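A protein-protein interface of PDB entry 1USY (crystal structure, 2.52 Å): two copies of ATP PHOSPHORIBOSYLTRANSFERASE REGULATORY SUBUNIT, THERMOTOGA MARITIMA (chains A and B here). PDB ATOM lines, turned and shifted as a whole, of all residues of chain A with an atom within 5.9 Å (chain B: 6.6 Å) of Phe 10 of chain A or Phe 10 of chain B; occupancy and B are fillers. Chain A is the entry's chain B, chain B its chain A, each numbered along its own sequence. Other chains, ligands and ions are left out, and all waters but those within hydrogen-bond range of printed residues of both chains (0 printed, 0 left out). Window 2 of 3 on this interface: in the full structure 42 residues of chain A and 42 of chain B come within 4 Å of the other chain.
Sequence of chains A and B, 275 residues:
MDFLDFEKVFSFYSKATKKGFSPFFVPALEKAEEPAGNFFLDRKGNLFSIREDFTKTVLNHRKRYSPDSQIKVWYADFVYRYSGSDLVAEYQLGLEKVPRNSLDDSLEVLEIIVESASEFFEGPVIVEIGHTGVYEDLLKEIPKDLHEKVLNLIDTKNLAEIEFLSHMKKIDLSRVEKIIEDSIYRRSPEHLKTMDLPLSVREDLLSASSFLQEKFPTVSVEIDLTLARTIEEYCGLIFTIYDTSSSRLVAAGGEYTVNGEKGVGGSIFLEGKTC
Phe 6 of chain A touches its own counterpart, Phe 6 of chain B. Phe 6 of chain A touches Tyr 13 of chain B, and with the chains exchanged Tyr 13 of chain A touches Phe 6 of chain B. Glu 7 of chain A touches Tyr 13 of chain B, but with the chains exchanged Tyr 13 of chain A does not touch Glu 7 of chain B (4.02 Å). Phe 10 of chain A touches its own counterpart, Phe 10 of chain B.
Of the printed residues of chain B, Glu 7 of chain A touches Tyr 13. Phe 10 of chain A touches just one residue of chain B: Phe 10 (3.1 Å). Of the printed residues of chain B, Tyr 13 of chain A touches Phe 6 (3.4 Å). Lys 15 of chain A touches none of the printed residues of chain B. Printed residues of chain A within 4 Å of Phe 6 of chain B: Phe 6 and Tyr 13. Printed residues of chain A within 4 Å of Val 9 of chain B: Phe 6 (3.8 Å). Of chain A, only Phe 10 (3.1 Å) comes within 4 Å of Phe 10 of chain B. Of the printed residues of chain A, Tyr 13 of chain B touches Phe 6 (3.3 Å) and Glu 7 (3.6 Å). Leu 93 of chain B touches none of the printed residues of chain A.
The backbone carbonyl oxygen of Phe 10 of chain B sits at hydrogen-bond distance from the side-chain hydroxyl of Ser 14 of chain B (3.3 Å). The backbone carbonyl oxygen (O) of Phe 10 of chain A lies within hydrogen-bond range of the side-chain hydroxyl (OG) of Ser 14 of chain A, 2.9 Å away.
Among the printed residues, merely in contact across the chains: Phe 6 of chain A with Phe 6 of chain B, Phe 6 of chain A with Val 9 of chain B, Phe 6 of chain A with Tyr 13 of chain B, Glu 7 of chain A with Tyr 13 of chain B, Phe 10 of chain A with Phe 10 of chain B and Tyr 13 of chain A with Phe 6 of chain B.
Of the 12 printed residues of chain B, 4 touch a printed residue of chain A. Hydrophobic or aromatic side chains of chain A within 4 Å of the printed part of chain B: Phe 6, Phe 10 and Tyr 13. Among the printed residues, 6 pairs touch across the chains. Among the printed residues, no Asp or Glu carboxylate lies within 4 Å of a Lys or Arg side-chain nitrogen of the other chain.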
ATOM      1  N   PHE A   6      21.127   3.713   1.636  1.00  0.00           N
ATOM      2  CA  PHE A   6      21.185   3.360   0.228  1.00  0.00           C
ATOM      3  C   PHE A   6      20.568   4.464  -0.641  1.00  0.00           C
ATOM      4  O   PHE A   6      20.880   4.543  -1.833  1.00  0.00           O
ATOM      5  CB  PHE A   6      20.469   2.045   0.022  1.00  0.00           C
ATOM      6  CG  PHE A   6      20.570   1.498  -1.358  1.00  0.00           C
ATOM      7  CD1 PHE A   6      19.576   1.782  -2.307  1.00  0.00           C
ATOM      8  CD2 PHE A   6      21.621   0.642  -1.699  1.00  0.00           C
ATOM      9  CE1 PHE A   6      19.633   1.247  -3.591  1.00  0.00           C
ATOM     10  CE2 PHE A   6      21.699   0.093  -2.987  1.00  0.00           C
ATOM     11  CZ  PHE A   6      20.698   0.407  -3.940  1.00  0.00           C
ATOM     12  N   GLU A   7      19.715   5.313  -0.049  1.00  0.00           N
ATOM     13  CA  GLU A   7      19.313   6.573  -0.668  1.00  0.00           C
ATOM     14  C   GLU A   7      20.554   7.300  -1.204  1.00  0.00           C
ATOM     15  O   GLU A   7      20.490   7.958  -2.244  1.00  0.00           O
ATOM     16  CB  GLU A   7      18.620   7.479   0.355  1.00  0.00           C
ATOM     17  CG  GLU A   7      17.184   7.881   0.025  1.00  0.00           C
ATOM     18  N   LYS A   8      21.675   7.188  -0.486  1.00  0.00           N
ATOM     19  CA  LYS A   8      22.900   7.904  -0.850  1.00  0.00           C
ATOM     20  C   LYS A   8      23.517   7.247  -2.080  1.00  0.00           C
ATOM     21  O   LYS A   8      23.964   7.925  -3.021  1.00  0.00           O
ATOM     22  CB  LYS A   8      23.878   7.995   0.328  1.00  0.00           C
ATOM     23  CG  LYS A   8      23.553   9.169   1.283  1.00  0.00           C
ATOM     24  CD  LYS A   8      24.323   9.153   2.623  1.00  0.00           C
ATOM     25  CE  LYS A   8      23.816  10.288   3.541  1.00  0.00           C
ATOM     26  NZ  LYS A   8      24.046  10.133   5.017  1.00  0.00           N
ATOM     27  N   VAL A   9      23.456   5.923  -2.096  1.00  0.00           N
ATOM     28  CA  VAL A   9      23.858   5.142  -3.265  1.00  0.00           C
ATOM     29  C   VAL A   9      22.999   5.436  -4.501  1.00  0.00           C
ATOM     30  O   VAL A   9      23.546   5.629  -5.571  1.00  0.00           O
ATOM     31  CB  VAL A   9      23.905   3.650  -2.961  1.00  0.00           C
ATOM     32  CG1 VAL A   9      24.606   2.953  -4.028  1.00  0.00           C
ATOM     33  CG2 VAL A   9      24.657   3.434  -1.664  1.00  0.00           C
ATOM     34  N   PHE A  10      21.678   5.504  -4.354  1.00  0.00           N
ATOM     35  CA  PHE A  10      20.801   5.832  -5.482  1.00  0.00           C
ATOM     36  C   PHE A  10      21.078   7.232  -6.013  1.00  0.00           C
ATOM     37  O   PHE A  10      21.136   7.456  -7.234  1.00  0.00           O
ATOM     38  CB  PHE A  10      19.324   5.746  -5.080  1.00  0.00           C
ATOM     39  CG  PHE A  10      18.366   6.319  -6.133  1.00  0.00           C
ATOM     40  CD1 PHE A  10      18.073   5.605  -7.306  1.00  0.00           C
ATOM     41  CD2 PHE A  10      17.766   7.563  -5.952  1.00  0.00           C
ATOM     42  CE1 PHE A  10      17.193   6.120  -8.263  1.00  0.00           C
ATOM     43  CE2 PHE A  10      16.895   8.086  -6.903  1.00  0.00           C
ATOM     44  CZ  PHE A  10      16.609   7.351  -8.065  1.00  0.00           C
ATOM     45  N   SER A  11      21.225   8.172  -5.077  1.00  0.00           N
ATOM     46  CA  SER A  11      21.488   9.557  -5.400  1.00  0.00           C
ATOM     47  C   SER A  11      22.762   9.709  -6.241  1.00  0.00           C
ATOM     48  O   SER A  11      22.739  10.379  -7.271  1.00  0.00           O
ATOM     49  CB  SER A  11      21.584  10.368  -4.107  1.00  0.00           C
ATOM     50  OG  SER A  11      21.923  11.730  -4.366  1.00  0.00           O
ATOM     51  N   PHE A  12      23.840   9.063  -5.791  1.00  0.00           N
ATOM     52  CA  PHE A  12      25.154   9.095  -6.427  1.00  0.00           C
ATOM     53  C   PHE A  12      25.090   8.489  -7.814  1.00  0.00           C
ATOM     54  O   PHE A  12      25.674   9.012  -8.739  1.00  0.00           O
ATOM     55  CB  PHE A  12      26.184   8.323  -5.574  1.00  0.00           C
ATOM     56  CG  PHE A  12      27.560   8.325  -6.153  1.00  0.00           C
ATOM     57  CD1 PHE A  12      28.371   9.460  -6.041  1.00  0.00           C
ATOM     58  CD2 PHE A  12      28.061   7.197  -6.792  1.00  0.00           C
ATOM     59  CE1 PHE A  12      29.644   9.480  -6.596  1.00  0.00           C
ATOM     60  CE2 PHE A  12      29.357   7.184  -7.339  1.00  0.00           C
ATOM     61  CZ  PHE A  12      30.146   8.334  -7.250  1.00  0.00           C
ATOM     62  N   TYR A  13      24.371   7.376  -7.919  1.00  0.00           N
ATOM     63  CA  TYR A  13      24.037   6.708  -9.169  1.00  0.00           C
ATOM     64  C   TYR A  13      23.266   7.635 -10.122  1.00  0.00           C
ATOM     65  O   TYR A  13      23.461   7.573 -11.335  1.00  0.00           O
ATOM     66  CB  TYR A  13      23.215   5.436  -8.852  1.00  0.00           C
ATOM     67  CG  TYR A  13      22.313   4.970  -9.982  1.00  0.00           C
ATOM     68  CD1 TYR A  13      22.858   4.480 -11.183  1.00  0.00           C
ATOM     69  CD2 TYR A  13      20.919   5.033  -9.866  1.00  0.00           C
ATOM     70  CE1 TYR A  13      22.052   4.073 -12.233  1.00  0.00           C
ATOM     71  CE2 TYR A  13      20.100   4.620 -10.923  1.00  0.00           C
ATOM     72  CZ  TYR A  13      20.678   4.139 -12.103  1.00  0.00           C
ATOM     73  OH  TYR A  13      19.888   3.713 -13.154  1.00  0.00           O
ATOM     74  N   SER A  14      22.377   8.479  -9.591  1.00  0.00           N
ATOM     75  CA  SER A  14      21.697   9.470 -10.441  1.00  0.00           C
ATOM     76  C   SER A  14      22.639  10.547 -10.919  1.00  0.00           C
ATOM     77  O   SER A  14      22.616  10.909 -12.081  1.00  0.00           O
ATOM     78  CB  SER A  14      20.470  10.092  -9.759  1.00  0.00           C
ATOM     79  OG  SER A  14      19.705   9.062  -9.156  1.00  0.00           O
ATOM     80  N   LYS A  15      23.467  11.058 -10.029  1.00  0.00           N
ATOM     81  CA  LYS A  15      24.450  12.048 -10.429  1.00  0.00           C
ATOM     82  C   LYS A  15      25.347  11.511 -11.524  1.00  0.00           C
ATOM     83  O   LYS A  15      25.583  12.212 -12.511  1.00  0.00           O
ATOM     84  CB  LYS A  15      25.280  12.520  -9.244  1.00  0.00           C
ATOM     85  CG  LYS A  15      24.466  13.244  -8.206  1.00  0.00           C
ATOM     86  CD  LYS A  15      25.284  13.482  -6.938  1.00  0.00           C
ATOM     87  CE  LYS A  15      24.392  13.732  -5.735  1.00  0.00           C
ATOM     88  NZ  LYS A  15      23.235  14.607  -6.056  1.00  0.00           N
ATOM     89  N   ASP B   5      22.513  -4.155 -14.466  1.00  0.00           N
ATOM     90  CA  ASP B   5      21.246  -3.423 -14.529  1.00  0.00           C
ATOM     91  C   ASP B   5      20.876  -2.869 -13.147  1.00  0.00           C
ATOM     92  O   ASP B   5      20.004  -3.388 -12.457  1.00  0.00           O
ATOM     93  CB  ASP B   5      20.106  -4.289 -15.079  1.00  0.00           C
ATOM     94  CG  ASP B   5      19.031  -3.471 -15.789  1.00  0.00           C
ATOM     95  OD1 ASP B   5      18.789  -2.276 -15.445  1.00  0.00           O
ATOM     96  OD2 ASP B   5      18.372  -3.948 -16.743  1.00  0.00           O
ATOM     97  N   PHE B   6      21.541  -1.796 -12.770  1.00  0.00           N
ATOM     98  CA  PHE B   6      21.231  -1.137 -11.530  1.00  0.00           C
ATOM     99  C   PHE B   6      19.769  -0.601 -11.497  1.00  0.00           C
ATOM    100  O   PHE B   6      19.175  -0.567 -10.435  1.00  0.00           O
ATOM    101  CB  PHE B   6      22.282  -0.059 -11.220  1.00  0.00           C
ATOM    102  CG  PHE B   6      22.238   0.467  -9.787  1.00  0.00           C
ATOM    103  CD1 PHE B   6      21.484   1.620  -9.468  1.00  0.00           C
ATOM    104  CD2 PHE B   6      22.955  -0.176  -8.767  1.00  0.00           C
ATOM    105  CE1 PHE B   6      21.449   2.103  -8.168  1.00  0.00           C
ATOM    106  CE2 PHE B   6      22.931   0.316  -7.465  1.00  0.00           C
ATOM    107  CZ  PHE B   6      22.182   1.453  -7.161  1.00  0.00           C
ATOM    108  N   GLU B   7      19.177  -0.209 -12.624  1.00  0.00           N
ATOM    109  CA  GLU B   7      17.770   0.215 -12.595  1.00  0.00           C
ATOM    110  C   GLU B   7      16.920  -0.856 -11.871  1.00  0.00           C
ATOM    111  O   GLU B   7      15.877  -0.554 -11.281  1.00  0.00           O
ATOM    112  CB  GLU B   7      17.212   0.534 -14.012  1.00  0.00           C
ATOM    113  CG  GLU B   7      16.389   1.838 -14.079  1.00  0.00           C
ATOM    114  CD  GLU B   7      15.760   2.151 -15.462  1.00  0.00           C
ATOM    115  OE1 GLU B   7      16.508   2.419 -16.439  1.00  0.00           O
ATOM    116  OE2 GLU B   7      14.502   2.165 -15.587  1.00  0.00           O
ATOM    117  N   LYS B   8      17.377  -2.107 -11.911  1.00  0.00           N
ATOM    118  CA  LYS B   8      16.644  -3.194 -11.271  1.00  0.00           C
ATOM    119  C   LYS B   8      16.864  -3.272  -9.768  1.00  0.00           C
ATOM    120  O   LYS B   8      15.936  -3.578  -9.015  1.00  0.00           O
ATOM    121  CB  LYS B   8      16.967  -4.534 -11.922  1.00  0.00           C
ATOM    122  CG  LYS B   8      16.156  -4.762 -13.183  1.00  0.00           C
ATOM    123  CD  LYS B   8      16.405  -6.115 -13.796  1.00  0.00           C
ATOM    124  CE  LYS B   8      15.971  -6.115 -15.266  1.00  0.00           C
ATOM    125  NZ  LYS B   8      17.100  -6.557 -16.128  1.00  0.00           N
ATOM    126  N   VAL B   9      18.088  -2.986  -9.331  1.00  0.00           N
ATOM    127  CA  VAL B   9      18.362  -2.938  -7.908  1.00  0.00           C
ATOM    128  C   VAL B   9      17.557  -1.828  -7.280  1.00  0.00           C
ATOM    129  O   VAL B   9      17.025  -2.022  -6.195  1.00  0.00           O
ATOM    130  CB  VAL B   9      19.843  -2.689  -7.583  1.00  0.00           C
ATOM    131  CG1 VAL B   9      20.035  -2.623  -6.061  1.00  0.00           C
ATOM    132  CG2 VAL B   9      20.703  -3.770  -8.204  1.00  0.00           C
ATOM    133  N   PHE B  10      17.485  -0.666  -7.944  1.00  0.00           N
ATOM    134  CA  PHE B  10      16.764   0.471  -7.400  1.00  0.00           C
ATOM    135  C   PHE B  10      15.288   0.148  -7.311  1.00  0.00           C
ATOM    136  O   PHE B  10      14.612   0.528  -6.356  1.00  0.00           O
ATOM    137  CB  PHE B  10      16.964   1.731  -8.238  1.00  0.00           C
ATOM    138  CG  PHE B  10      15.922   2.823  -7.951  1.00  0.00           C
ATOM    139  CD1 PHE B  10      15.887   3.466  -6.704  1.00  0.00           C
ATOM    140  CD2 PHE B  10      14.963   3.163  -8.899  1.00  0.00           C
ATOM    141  CE1 PHE B  10      14.932   4.446  -6.422  1.00  0.00           C
ATOM    142  CE2 PHE B  10      14.009   4.127  -8.620  1.00  0.00           C
ATOM    143  CZ  PHE B  10      13.997   4.781  -7.380  1.00  0.00           C
ATOM    144  N   SER B  11      14.782  -0.549  -8.318  1.00  0.00           N
ATOM    145  CA  SER B  11      13.380  -0.973  -8.350  1.00  0.00           C
ATOM    146  C   SER B  11      13.061  -1.884  -7.145  1.00  0.00           C
ATOM    147  O   SER B  11      12.094  -1.694  -6.397  1.00  0.00           O
ATOM    148  CB  SER B  11      13.124  -1.713  -9.652  1.00  0.00           C
ATOM    149  OG  SER B  11      11.757  -2.009  -9.788  1.00  0.00           O
ATOM    150  N   PHE B  12      13.934  -2.849  -6.961  1.00  0.00           N
ATOM    151  CA  PHE B  12      13.816  -3.782  -5.889  1.00  0.00           C
ATOM    152  C   PHE B  12      13.830  -3.008  -4.583  1.00  0.00           C
ATOM    153  O   PHE B  12      12.977  -3.246  -3.714  1.00  0.00           O
ATOM    154  CB  PHE B  12      14.975  -4.795  -5.920  1.00  0.00           C
ATOM    155  CG  PHE B  12      14.847  -5.841  -4.872  1.00  0.00           C
ATOM    156  CD1 PHE B  12      13.787  -6.755  -4.922  1.00  0.00           C
ATOM    157  CD2 PHE B  12      15.751  -5.899  -3.813  1.00  0.00           C
ATOM    158  CE1 PHE B  12      13.635  -7.708  -3.936  1.00  0.00           C
ATOM    159  CE2 PHE B  12      15.614  -6.872  -2.818  1.00  0.00           C
ATOM    160  CZ  PHE B  12      14.559  -7.771  -2.873  1.00  0.00           C
ATOM    161  N   TYR B  13      14.797  -2.088  -4.469  1.00  0.00           N
ATOM    162  CA  TYR B  13      15.003  -1.256  -3.278  1.00  0.00           C
ATOM    163  C   TYR B  13      13.700  -0.519  -2.950  1.00  0.00           C
ATOM    164  O   TYR B  13      13.197  -0.659  -1.851  1.00  0.00           O
ATOM    165  CB  TYR B  13      16.234  -0.324  -3.430  1.00  0.00           C
ATOM    166  CG  TYR B  13      16.174   0.988  -2.626  1.00  0.00           C
ATOM    167  CD1 TYR B  13      16.508   1.035  -1.248  1.00  0.00           C
ATOM    168  CD2 TYR B  13      15.774   2.173  -3.232  1.00  0.00           C
ATOM    169  CE1 TYR B  13      16.435   2.251  -0.527  1.00  0.00           C
ATOM    170  CE2 TYR B  13      15.700   3.350  -2.519  1.00  0.00           C
ATOM    171  CZ  TYR B  13      16.030   3.386  -1.182  1.00  0.00           C
ATOM    172  OH  TYR B  13      15.949   4.589  -0.527  1.00  0.00           O
ATOM    173  N   SER B  14      13.113   0.183  -3.908  1.00  0.00           N
ATOM    174  CA  SER B  14      11.840   0.847  -3.665  1.00  0.00           C
ATOM    175  C   SER B  14      10.779  -0.124  -3.189  1.00  0.00           C
ATOM    176  O   SER B  14      10.033   0.170  -2.261  1.00  0.00           O
ATOM    177  CB  SER B  14      11.312   1.557  -4.917  1.00  0.00           C
ATOM    178  OG  SER B  14      12.198   2.562  -5.363  1.00  0.00           O
ATOM    179  N   LYS B  15      10.678  -1.261  -3.851  1.00  0.00           N
ATOM    180  CA  LYS B  15       9.696  -2.260  -3.459  1.00  0.00           C
ATOM    181  C   LYS B  15       9.856  -2.669  -1.988  1.00  0.00           C
ATOM    182  O   LYS B  15       8.864  -2.657  -1.236  1.00  0.00           O
ATOM    183  CB  LYS B  15       9.804  -3.495  -4.348  1.00  0.00           C
ATOM    184  CG  LYS B  15       9.356  -3.203  -5.753  1.00  0.00           C
ATOM    185  CD  LYS B  15       9.211  -4.456  -6.548  1.00  0.00           C
ATOM    186  CE  LYS B  15       8.467  -4.114  -7.815  1.00  0.00           C
ATOM    187  NZ  LYS B  15       9.423  -3.573  -8.792  1.00  0.00           N
ATOM    188  N   LEU B  93      19.433 -10.336  -5.244  1.00  0.00           N
ATOM    189  CA  LEU B  93      18.566  -9.430  -4.543  1.00  0.00           C
ATOM    190  C   LEU B  93      17.749 -10.313  -3.603  1.00  0.00           C
ATOM    191  O   LEU B  93      17.088 -11.228  -4.048  1.00  0.00           O
ATOM    192  CB  LEU B  93      17.645  -8.676  -5.534  1.00  0.00           C
ATOM    193  CG  LEU B  93      18.371  -7.764  -6.529  1.00  0.00           C
ATOM    194  CD1 LEU B  93      17.442  -7.212  -7.624  1.00  0.00           C
ATOM    195  CD2 LEU B  93      19.014  -6.596  -5.758  1.00  0.00           C
